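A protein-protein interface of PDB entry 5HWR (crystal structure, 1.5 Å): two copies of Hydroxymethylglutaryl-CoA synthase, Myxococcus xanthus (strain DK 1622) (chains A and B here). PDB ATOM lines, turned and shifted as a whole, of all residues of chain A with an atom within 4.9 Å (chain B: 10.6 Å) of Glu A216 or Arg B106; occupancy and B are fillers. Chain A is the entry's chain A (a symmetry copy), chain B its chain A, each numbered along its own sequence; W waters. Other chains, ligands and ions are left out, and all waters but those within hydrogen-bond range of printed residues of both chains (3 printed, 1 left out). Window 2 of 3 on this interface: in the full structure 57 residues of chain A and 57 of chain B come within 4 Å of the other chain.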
ATOM      1  N   VAL A 186      32.101  23.333  33.025  1.00  0.00           N
ATOM      2  CA  VAL A 186      30.884  23.511  32.238  1.00  0.00           C
ATOM      3  C   VAL A 186      31.077  24.623  31.208  1.00  0.00           C
ATOM      4  O   VAL A 186      31.826  25.581  31.422  1.00  0.00           O
ATOM      5  CB  VAL A 186      29.690  23.773  33.183  1.00  0.00           C
ATOM      6  CG1 VAL A 186      29.827  25.098  33.860  1.00  0.00           C
ATOM      7  CG2 VAL A 186      28.344  23.552  32.487  1.00  0.00           C
ATOM      8  N   CYS A 187      30.405  24.466  30.070  1.00  0.00           N
ATOM      9  CA  CYS A 187      30.435  25.466  29.009  1.00  0.00           C
ATOM     10  C   CYS A 187      29.101  25.444  28.281  1.00  0.00           C
ATOM     11  O   CYS A 187      28.725  24.417  27.718  1.00  0.00           O
ATOM     12  CB  CYS A 187      31.573  25.166  28.040  1.00  0.00           C
ATOM     13  SG  CYS A 187      31.742  26.340  26.703  1.00  0.00           S
ATOM     14  N   SER A 188      28.405  26.568  28.280  1.00  0.00           N
ATOM     15  CA  SER A 188      27.079  26.655  27.682  1.00  0.00           C
ATOM     16  C   SER A 188      26.940  27.959  26.911  1.00  0.00           C
ATOM     17  O   SER A 188      27.473  28.999  27.308  1.00  0.00           O
ATOM     18  CB  SER A 188      25.984  26.542  28.753  1.00  0.00           C
ATOM     19  OG  SER A 188      26.193  27.544  29.694  1.00  0.00           O
ATOM     20  N   MET A 189      26.197  27.888  25.815  1.00  0.00           N
ATOM     21  CA  MET A 189      25.885  29.081  25.045  1.00  0.00           C
ATOM     22  C   MET A 189      24.660  28.813  24.188  1.00  0.00           C
ATOM     23  O   MET A 189      24.376  27.675  23.828  1.00  0.00           O
ATOM     24  CB  MET A 189      27.054  29.541  24.182  1.00  0.00           C
ATOM     25  CG  MET A 189      27.539  28.477  23.228  1.00  0.00           C
ATOM     26  SD  MET A 189      28.817  27.431  23.968  1.00  0.00           S
ATOM     27  CE  MET A 189      29.470  26.699  22.463  1.00  0.00           C
ATOM     28  N   THR A 212      30.440  20.988  15.474  1.00  0.00           N
ATOM     29  CA  THR A 212      31.319  22.074  15.906  1.00  0.00           C
ATOM     30  C   THR A 212      30.926  22.587  17.282  1.00  0.00           C
ATOM     31  O   THR A 212      31.791  22.867  18.113  1.00  0.00           O
ATOM     32  CB  THR A 212      31.301  23.197  14.884  1.00  0.00           C
ATOM     33  OG1 THR A 212      31.752  22.661  13.640  1.00  0.00           O
ATOM     34  CG2 THR A 212      32.222  24.377  15.326  1.00  0.00           C
ATOM     35  N   CYS A 213      29.616  22.693  17.555  1.00  0.00           N
ATOM     36  CA  CYS A 213      29.188  23.175  18.864  1.00  0.00           C
ATOM     37  C   CYS A 213      29.563  22.175  19.948  1.00  0.00           C
ATOM     38  O   CYS A 213      30.003  22.558  21.031  1.00  0.00           O
ATOM     39  CB  CYS A 213      27.692  23.430  18.884  1.00  0.00           C
ATOM     40  SG  CYS A 213      27.154  24.852  17.890  1.00  0.00           S
ATOM     41  N   TYR A 214      29.343  20.891  19.686  1.00  0.00           N
ATOM     42  CA  TYR A 214      29.767  19.850  20.619  1.00  0.00           C
ATOM     43  C   TYR A 214      31.240  19.985  20.967  1.00  0.00           C
ATOM     44  O   TYR A 214      31.617  20.010  22.144  1.00  0.00           O
ATOM     45  CB  TYR A 214      29.465  18.482  20.016  1.00  0.00           C
ATOM     46  CG  TYR A 214      29.860  17.226  20.811  1.00  0.00           C
ATOM     47  CD1 TYR A 214      31.150  17.004  21.250  1.00  0.00           C
ATOM     48  CD2 TYR A 214      28.932  16.208  21.035  1.00  0.00           C
ATOM     49  CE1 TYR A 214      31.491  15.828  21.894  1.00  0.00           C
ATOM     50  CE2 TYR A 214      29.283  15.018  21.687  1.00  0.00           C
ATOM     51  CZ  TYR A 214      30.552  14.849  22.120  1.00  0.00           C
ATOM     52  OH  TYR A 214      30.967  13.706  22.770  1.00  0.00           O
ATOM     53  N   LEU A 215      32.095  20.103  19.945  1.00  0.00           N
ATOM     54  CA  LEU A 215      33.527  20.144  20.194  1.00  0.00           C
ATOM     55  C   LEU A 215      33.936  21.442  20.888  1.00  0.00           C
ATOM     56  O   LEU A 215      34.839  21.443  21.745  1.00  0.00           O
ATOM     57  CB  LEU A 215      34.289  19.935  18.882  1.00  0.00           C
ATOM     58  CG  LEU A 215      34.046  18.564  18.260  1.00  0.00           C
ATOM     59  CD1 LEU A 215      34.656  18.496  16.885  1.00  0.00           C
ATOM     60  CD2 LEU A 215      34.538  17.380  19.130  1.00  0.00           C
ATOM     61  N   GLU A 216      33.276  22.553  20.550  1.00  0.00           N
ATOM     62  CA  GLU A 216      33.557  23.825  21.218  1.00  0.00           C
ATOM     63  C   GLU A 216      33.182  23.756  22.690  1.00  0.00           C
ATOM     64  O   GLU A 216      33.957  24.154  23.576  1.00  0.00           O
ATOM     65  CB  GLU A 216      32.791  24.966  20.525  1.00  0.00           C
ATOM     66  CG  GLU A 216      33.053  26.307  21.148  1.00  0.00           C
ATOM     67  CD  GLU A 216      32.419  27.444  20.411  1.00  0.00           C
ATOM     68  OE1 GLU A 216      31.590  27.211  19.490  1.00  0.00           O
ATOM     69  OE2 GLU A 216      32.766  28.600  20.757  1.00  0.00           O
ATOM     70  N   ALA A 217      31.967  23.283  22.977  1.00  0.00           N
ATOM     71  CA  ALA A 217      31.526  23.189  24.360  1.00  0.00           C
ATOM     72  C   ALA A 217      32.347  22.171  25.149  1.00  0.00           C
ATOM     73  O   ALA A 217      32.659  22.401  26.325  1.00  0.00           O
ATOM     74  CB  ALA A 217      30.029  22.873  24.398  1.00  0.00           C
ATOM     75  N   LEU A 218      32.686  21.044  24.538  1.00  0.00           N
ATOM     76  CA  LEU A 218      33.575  20.073  25.174  1.00  0.00           C
ATOM     77  C   LEU A 218      34.869  20.736  25.606  1.00  0.00           C
ATOM     78  O   LEU A 218      35.349  20.534  26.726  1.00  0.00           O
ATOM     79  CB  LEU A 218      33.841  18.912  24.200  1.00  0.00           C
ATOM     80  CG  LEU A 218      34.888  17.889  24.632  1.00  0.00           C
ATOM     81  CD1 LEU A 218      34.665  16.603  23.833  1.00  0.00           C
ATOM     82  CD2 LEU A 218      36.349  18.351  24.407  1.00  0.00           C
ATOM     83  N   SER A 219      35.466  21.534  24.711  1.00  0.00           N
ATOM     84  CA  SER A 219      36.752  22.156  25.021  1.00  0.00           C
ATOM     85  C   SER A 219      36.656  23.034  26.268  1.00  0.00           C
ATOM     86  O   SER A 219      37.527  22.998  27.149  1.00  0.00           O
ATOM     87  CB  SER A 219      37.226  22.980  23.820  1.00  0.00           C
ATOM     88  OG  SER A 219      37.457  22.163  22.682  1.00  0.00           O
ATOM     89  N   GLY A 220      35.617  23.861  26.336  1.00  0.00           N
ATOM     90  CA  GLY A 220      35.447  24.717  27.495  1.00  0.00           C
ATOM     91  C   GLY A 220      35.172  23.926  28.762  1.00  0.00           C
ATOM     92  O   GLY A 220      35.707  24.238  29.829  1.00  0.00           O
ATOM     93  N   ASP B  73      27.174  40.285  39.221  1.00  0.00           N
ATOM     94  CA  ASP B  73      28.254  40.064  38.266  1.00  0.00           C
ATOM     95  C   ASP B  73      27.879  38.814  37.480  1.00  0.00           C
ATOM     96  O   ASP B  73      27.880  37.727  38.053  1.00  0.00           O
ATOM     97  CB  ASP B  73      29.582  39.870  38.992  1.00  0.00           C
ATOM     98  CG  ASP B  73      30.736  39.568  38.076  1.00  0.00           C
ATOM     99  OD1 ASP B  73      30.582  39.081  36.950  1.00  0.00           O
ATOM    100  OD2 ASP B  73      31.855  39.813  38.522  1.00  0.00           O
ATOM    101  N   PRO B  74      27.525  38.931  36.196  1.00  0.00           N
ATOM    102  CA  PRO B  74      27.046  37.764  35.434  1.00  0.00           C
ATOM    103  C   PRO B  74      28.027  36.613  35.414  1.00  0.00           C
ATOM    104  O   PRO B  74      27.617  35.442  35.307  1.00  0.00           O
ATOM    105  CB  PRO B  74      26.838  38.341  34.025  1.00  0.00           C
ATOM    106  CG  PRO B  74      26.771  39.793  34.204  1.00  0.00           C
ATOM    107  CD  PRO B  74      27.535  40.161  35.387  1.00  0.00           C
ATOM    108  N   SER B  75      29.322  36.900  35.516  1.00  0.00           N
ATOM    109  CA  SER B  75      30.310  35.836  35.470  1.00  0.00           C
ATOM    110  C   SER B  75      30.383  35.030  36.763  1.00  0.00           C
ATOM    111  O   SER B  75      31.074  33.992  36.803  1.00  0.00           O
ATOM    112  CB  SER B  75      31.699  36.398  35.120  1.00  0.00           C
ATOM    113  OG  SER B  75      32.280  37.118  36.183  1.00  0.00           O
ATOM    114  N   ARG B  76      29.655  35.448  37.801  1.00  0.00           N
ATOM    115  CA  ARG B  76      29.555  34.649  39.016  1.00  0.00           C
ATOM    116  C   ARG B  76      28.421  33.630  38.952  1.00  0.00           C
ATOM    117  O   ARG B  76      28.284  32.832  39.882  1.00  0.00           O
ATOM    118  CB  ARG B  76      29.386  35.568  40.236  1.00  0.00           C
ATOM    119  CG  ARG B  76      30.616  36.484  40.444  1.00  0.00           C
ATOM    120  CD  ARG B  76      30.538  37.268  41.704  1.00  0.00           C
ATOM    121  NE  ARG B  76      30.609  36.343  42.826  1.00  0.00           N
ATOM    122  CZ  ARG B  76      29.683  36.192  43.758  1.00  0.00           C
ATOM    123  NH1 ARG B  76      28.584  36.952  43.770  1.00  0.00           N
ATOM    124  NH2 ARG B  76      29.870  35.269  44.700  1.00  0.00           N
ATOM    125  N   ILE B  77      27.580  33.684  37.921  1.00  0.00           N
ATOM    126  CA  ILE B  77      26.467  32.754  37.793  1.00  0.00           C
ATOM    127  C   ILE B  77      27.007  31.413  37.298  1.00  0.00           C
ATOM    128  O   ILE B  77      27.593  31.335  36.210  1.00  0.00           O
ATOM    129  CB  ILE B  77      25.408  33.295  36.832  1.00  0.00           C
ATOM    130  CG1 ILE B  77      24.858  34.637  37.332  1.00  0.00           C
ATOM    131  CG2 ILE B  77      24.275  32.269  36.644  1.00  0.00           C
ATOM    132  CD1 ILE B  77      24.020  35.378  36.291  1.00  0.00           C
ATOM    133  N   GLY B  78      26.810  30.364  38.101  1.00  0.00           N
ATOM    134  CA  GLY B  78      27.212  29.011  37.741  1.00  0.00           C
ATOM    135  C   GLY B  78      26.086  28.064  37.370  1.00  0.00           C
ATOM    136  O   GLY B  78      26.335  26.952  36.894  1.00  0.00           O
ATOM    137  N   MET B  79      24.853  28.515  37.577  1.00  0.00           N
ATOM    138  CA  MET B  79      23.654  27.749  37.228  1.00  0.00           C
ATOM    139  C   MET B  79      22.571  28.740  36.840  1.00  0.00           C
ATOM    140  O   MET B  79      22.322  29.694  37.577  1.00  0.00           O
ATOM    141  CB  MET B  79      23.111  26.902  38.389  1.00  0.00           C
ATOM    142  CG  MET B  79      23.895  25.689  38.734  1.00  0.00           C
ATOM    143  SD  MET B  79      23.112  24.679  40.019  1.00  0.00           S
ATOM    144  CE  MET B  79      21.690  24.035  39.192  1.00  0.00           C
ATOM    145  N   LEU B  80      21.917  28.487  35.711  1.00  0.00           N
ATOM    146  CA  LEU B  80      20.742  29.232  35.253  1.00  0.00           C
ATOM    147  C   LEU B  80      19.689  28.181  34.949  1.00  0.00           C
ATOM    148  O   LEU B  80      19.838  27.411  33.990  1.00  0.00           O
ATOM    149  CB  LEU B  80      21.053  30.085  34.013  1.00  0.00           C
ATOM    150  CG  LEU B  80      19.868  30.814  33.354  1.00  0.00           C
ATOM    151  CD1 LEU B  80      19.261  31.840  34.297  1.00  0.00           C
ATOM    152  CD2 LEU B  80      20.284  31.471  32.072  1.00  0.00           C
ATOM    153  N   ALA B  95      15.997  28.229  29.479  1.00  0.00           N
ATOM    154  CA  ALA B  95      17.225  28.730  30.091  1.00  0.00           C
ATOM    155  C   ALA B  95      18.296  29.080  29.057  1.00  0.00           C
ATOM    156  O   ALA B  95      19.050  30.030  29.250  1.00  0.00           O
ATOM    157  CB  ALA B  95      17.790  27.710  31.055  1.00  0.00           C
ATOM    158  N   SER B  96      18.407  28.313  27.975  1.00  0.00           N
ATOM    159  CA  SER B  96      19.411  28.645  26.950  1.00  0.00           C
ATOM    160  C   SER B  96      19.064  29.920  26.207  1.00  0.00           C
ATOM    161  O   SER B  96      19.958  30.721  25.900  1.00  0.00           O
ATOM    162  CB  SER B  96      19.619  27.487  25.965  1.00  0.00           C
ATOM    163  OG  SER B  96      18.540  27.260  25.090  1.00  0.00           O
ATOM    164  N   GLN B  99      19.926  32.801  28.557  1.00  0.00           N
ATOM    165  CA  GLN B  99      21.373  33.005  28.556  1.00  0.00           C
ATOM    166  C   GLN B  99      21.796  33.862  27.385  1.00  0.00           C
ATOM    167  O   GLN B  99      22.599  34.790  27.536  1.00  0.00           O
ATOM    168  CB  GLN B  99      22.093  31.662  28.491  1.00  0.00           C
ATOM    169  CG  GLN B  99      23.588  31.768  28.524  1.00  0.00           C
ATOM    170  CD  GLN B  99      24.261  30.413  28.437  1.00  0.00           C
ATOM    171  OE1 GLN B  99      23.875  29.550  27.650  1.00  0.00           O
ATOM    172  NE2 GLN B  99      25.291  30.241  29.219  1.00  0.00           N
ATOM    173  N   GLY B 100      21.309  33.528  26.186  1.00  0.00           N
ATOM    174  CA  GLY B 100      21.704  34.308  25.017  1.00  0.00           C
ATOM    175  C   GLY B 100      21.148  35.722  25.019  1.00  0.00           C
ATOM    176  O   GLY B 100      21.848  36.684  24.650  1.00  0.00           O
ATOM    177  N   LEU B 102      20.388  37.610  27.501  1.00  0.00           N
ATOM    178  CA  LEU B 102      21.109  38.393  28.492  1.00  0.00           C
ATOM    179  C   LEU B 102      22.598  38.496  28.200  1.00  0.00           C
ATOM    180  O   LEU B 102      23.321  39.169  28.959  1.00  0.00           O
ATOM    181  CB  LEU B 102      20.897  37.785  29.869  1.00  0.00           C
ATOM    182  CG  LEU B 102      19.635  38.258  30.592  1.00  0.00           C
ATOM    183  CD1 LEU B 102      18.360  38.039  29.778  1.00  0.00           C
ATOM    184  CD2 LEU B 102      19.499  37.559  31.932  1.00  0.00           C
ATOM    185  N   LYS B 103      23.087  37.828  27.162  1.00  0.00           N
ATOM    186  CA  LYS B 103      24.507  37.846  26.834  1.00  0.00           C
ATOM    187  C   LYS B 103      25.359  37.356  28.010  1.00  0.00           C
ATOM    188  O   LYS B 103      26.413  37.907  28.324  1.00  0.00           O
ATOM    189  CB  LYS B 103      24.936  39.237  26.362  1.00  0.00           C
ATOM    190  CG  LYS B 103      24.089  39.787  25.206  1.00  0.00           C
ATOM    191  CD  LYS B 103      24.361  41.259  24.889  1.00  0.00           C
ATOM    192  CE  LYS B 103      23.452  41.799  23.792  1.00  0.00           C
ATOM    193  NZ  LYS B 103      23.805  43.185  23.441  1.00  0.00           N
ATOM    194  N   LEU B 104      24.877  36.333  28.701  1.00  0.00           N
ATOM    195  CA  LEU B 104      25.623  35.775  29.798  1.00  0.00           C
ATOM    196  C   LEU B 104      26.801  34.946  29.302  1.00  0.00           C
ATOM    197  O   LEU B 104      26.742  34.355  28.215  1.00  0.00           O
ATOM    198  CB  LEU B 104      24.725  34.879  30.638  1.00  0.00           C
ATOM    199  CG  LEU B 104      23.497  35.569  31.243  1.00  0.00           C
ATOM    200  CD1 LEU B 104      22.704  34.584  32.095  1.00  0.00           C
ATOM    201  CD2 LEU B 104      23.905  36.765  32.066  1.00  0.00           C
ATOM    202  N   PRO B 105      27.862  34.852  30.113  1.00  0.00           N
ATOM    203  CA  PRO B 105      29.017  34.029  29.755  1.00  0.00           C
ATOM    204  C   PRO B 105      28.753  32.531  29.891  1.00  0.00           C
ATOM    205  O   PRO B 105      27.628  32.099  30.178  1.00  0.00           O
ATOM    206  CB  PRO B 105      30.111  34.555  30.706  1.00  0.00           C
ATOM    207  CG  PRO B 105      29.380  35.053  31.923  1.00  0.00           C
ATOM    208  CD  PRO B 105      28.076  35.611  31.361  1.00  0.00           C
ATOM    209  N   ARG B 106      29.795  31.737  29.652  1.00  0.00           N
ATOM    210  CA  ARG B 106      29.630  30.319  29.351  1.00  0.00           C
ATOM    211  C   ARG B 106      29.753  29.381  30.531  1.00  0.00           C
ATOM    212  O   ARG B 106      29.362  28.206  30.397  1.00  0.00           O
ATOM    213  CB  ARG B 106      30.661  29.888  28.294  1.00  0.00           C
ATOM    214  CG  ARG B 106      30.412  30.586  26.990  1.00  0.00           C
ATOM    215  CD  ARG B 106      31.381  30.177  25.898  1.00  0.00           C
ATOM    216  NE  ARG B 106      30.900  30.643  24.606  1.00  0.00           N
ATOM    217  CZ  ARG B 106      31.355  30.197  23.448  1.00  0.00           C
ATOM    218  NH1 ARG B 106      32.335  29.316  23.418  1.00  0.00           N
ATOM    219  NH2 ARG B 106      30.798  30.623  22.330  1.00  0.00           N
ATOM    220  N   THR B 107      30.297  29.821  31.667  1.00  0.00           N
ATOM    221  CA  THR B 107      30.628  28.873  32.733  1.00  0.00           C
ATOM    222  C   THR B 107      29.450  28.680  33.683  1.00  0.00           C
ATOM    223  O   THR B 107      29.506  28.992  34.885  1.00  0.00           O
ATOM    224  CB  THR B 107      31.864  29.315  33.497  1.00  0.00           C
ATOM    225  OG1 THR B 107      32.877  29.748  32.573  1.00  0.00           O
ATOM    226  CG2 THR B 107      32.385  28.147  34.357  1.00  0.00           C
ATOM    227  N   MET B 108      28.372  28.144  33.120  1.00  0.00           N
ATOM    228  CA  MET B 108      27.191  27.829  33.917  1.00  0.00           C
ATOM    229  C   MET B 108      26.454  26.637  33.319  1.00  0.00           C
ATOM    230  O   MET B 108      26.403  26.442  32.102  1.00  0.00           O
ATOM    231  CB  MET B 108      26.222  29.030  34.012  1.00  0.00           C
ATOM    232  CG  MET B 108      25.765  29.558  32.648  1.00  0.00           C
ATOM    233  SD  MET B 108      24.796  31.072  32.771  1.00  0.00           S
ATOM    234  CE  MET B 108      26.073  32.230  33.226  1.00  0.00           C
ATOM    235  N   ARG B 109      25.845  25.856  34.212  1.00  0.00           N
ATOM    236  CA  ARG B 109      24.810  24.904  33.811  1.00  0.00           C
ATOM    237  C   ARG B 109      23.591  25.677  33.360  1.00  0.00           C
ATOM    238  O   ARG B 109      23.232  26.675  33.975  1.00  0.00           O
ATOM    239  CB  ARG B 109      24.396  23.993  34.982  1.00  0.00           C
ATOM    240  CG  ARG B 109      25.488  23.158  35.613  1.00  0.00           C
ATOM    241  CD  ARG B 109      24.920  22.218  36.643  1.00  0.00           C
ATOM    242  NE  ARG B 109      26.004  21.530  37.316  1.00  0.00           N
ATOM    243  CZ  ARG B 109      26.000  21.147  38.581  1.00  0.00           C
ATOM    244  NH1 ARG B 109      24.927  21.312  39.326  1.00  0.00           N
ATOM    245  NH2 ARG B 109      27.077  20.581  39.096  1.00  0.00           N
ATOM    246  N   THR B 110      22.947  25.211  32.295  1.00  0.00           N
ATOM    247  CA  THR B 110      21.646  25.728  31.884  1.00  0.00           C
ATOM    248  C   THR B 110      20.693  24.556  31.671  1.00  0.00           C
ATOM    249  O   THR B 110      21.055  23.562  31.038  1.00  0.00           O
ATOM    250  CB  THR B 110      21.722  26.569  30.618  1.00  0.00           C
ATOM    251  OG1 THR B 110      22.184  25.792  29.520  1.00  0.00           O
ATOM    252  CG2 THR B 110      22.638  27.743  30.782  1.00  0.00           C
ATOM    253  N   LYS B 139      30.031  31.057  44.070  1.00  0.00           N
ATOM    254  CA  LYS B 139      29.244  31.406  42.890  1.00  0.00           C
ATOM    255  C   LYS B 139      27.789  31.593  43.307  1.00  0.00           C
ATOM    256  O   LYS B 139      27.426  31.358  44.457  1.00  0.00           O
ATOM    257  CB  LYS B 139      29.390  30.331  41.806  1.00  0.00           C
ATOM    258  CG  LYS B 139      30.795  30.366  41.073  1.00  0.00           C
ATOM    259  CD  LYS B 139      30.663  29.920  39.624  1.00  0.00           C
ATOM    260  CE  LYS B 139      31.828  30.073  38.789  1.00  0.00           C
ATOM    261  NZ  LYS B 139      31.494  29.419  37.444  1.00  0.00           N
HETATM  262  O   HOH W   1      34.355  28.573  25.326  1.00  0.00           O
HETATM  263  O   HOH W   2      33.109  27.626  30.324  1.00  0.00           O
HETATM  264  O   HOH W   3      30.043  29.585  19.483  1.00  0.00           O
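N of Met A189 lies close to OE1 of Gln B99, 3.4 Å away.
O of Arg B106 lies within hydrogen-bond range of N of Ser A188.
NE2 of Gln B99 lies within hydrogen-bond range of OG of Ser A188 (2.9 Å).
OG of Ser A188 lies within hydrogen-bond range of O of Met B108.
The guanidinium group (NH1) of Arg B106 is in salt-bridge range of the side-chain carboxylate (OE2) of Glu A216 (2.8 Å).
The backbone carbonyl oxygen (O) of Gly B78 sits at hydrogen-bond distance from the backbone NH (N) of Arg B109 (2.9 Å).
The backbone carbonyl oxygen (O) of Pro B105 sits at hydrogen-bond distance from the side-chain amide nitrogen (NE2) of Gln B99, at 3.1 Å.
SD of Met B108 lies close to NE2 of Gln B99 (3.7 Å).
O of Arg B109 is in hydrogen-bond range of N of Leu B80, at 2.8 Å.
NZ of Lys B139 is in hydrogen-bond range of O of Thr B107 (3.3 Å).
The backbone carbonyl oxygen of Gln B99 is in hydrogen-bond range of the backbone NH of Leu B104 (3.0 Å).
Arg B106 touches Val A186 (O to O, 3.7 Å).
Thr B107 touches Val A186 (C to CG1, 3.6 Å).
N of Met B108 touches CG1 of Val A186 (3.5 Å).
Val A186 touches Arg B109 (CG2 to N, 3.8 Å).
Cys A187 touches Arg B106 (CA to O, 3.3 Å).
Ser A188 touches Thr B110.
SD of Met A189 touches CZ of Arg B106 (3.8 Å).
Of the printed residues of chain B, Val A186 touches Arg B106, Thr B107, Met B108 and Arg B109.
Of chain B, only Gln B99, Arg B106, Met B108 and Thr B110 come within 4 Å of Ser A188.
Of the printed residues of chain B, Met A189 touches Gln B99 and Arg B106.
No residue of chain B comes within 4 Å of Cys A213.
Glu A216 touches one residue of chain B.
No residue of chain B comes within 4 Å of Ser A219.
Gly A220 touches none of the printed residues of chain B.
Leu B80 touches none of the printed residues of chain A.
Arg B106 touches five residues of chain A.
Printed residues of chain A within 4 Å of Met B108: Val A186 (3.5 Å) and Ser A188 (2.7 Å).
Of the 13 printed residues of chain A, 5 touch a printed residue of chain B.
Printed residues of chain A that touch a printed residue of chain B: Val A186, Cys A187, Ser A188, Met A189 and Glu A216.
Hydrophobic or aromatic side chains of chain A within 4 Å of the printed part of chain B: Val A186 and Met A189.
Along chain A the printed residues that touch a printed residue of chain B span positions 186 to 216.
Hydrophobic or aromatic side chains of chain B within 4 Å of the printed part of chain A: Met B108.
Along chain B the printed residues that touch a printed residue of chain A span positions 99 to 110.
Among the printed residues, 12 pairs touch across the chains.
Among the printed residues, Asp or Glu carboxylates within 4 Å of a Lys or Arg side-chain nitrogen of the other chain: Glu A216 with Arg B106 (2.8 Å).
No position is printed for both chains.
Water W2 bridges the backbone carbonyl oxygen (O) of Val A186 (2.7 Å) and the side-chain hydroxyl (OG1) of Thr B107 (3.1 Å).
Water W3 lies within hydrogen-bond range of the side-chain carboxylate of Glu A216 (2.8 Å) and the guanidinium group of Arg B106 (3.1 Å).
Water W1 lies within hydrogen-bond range of NH1 of Arg B106 (2.9 Å) and SG of Cys A187 (3.7 Å).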
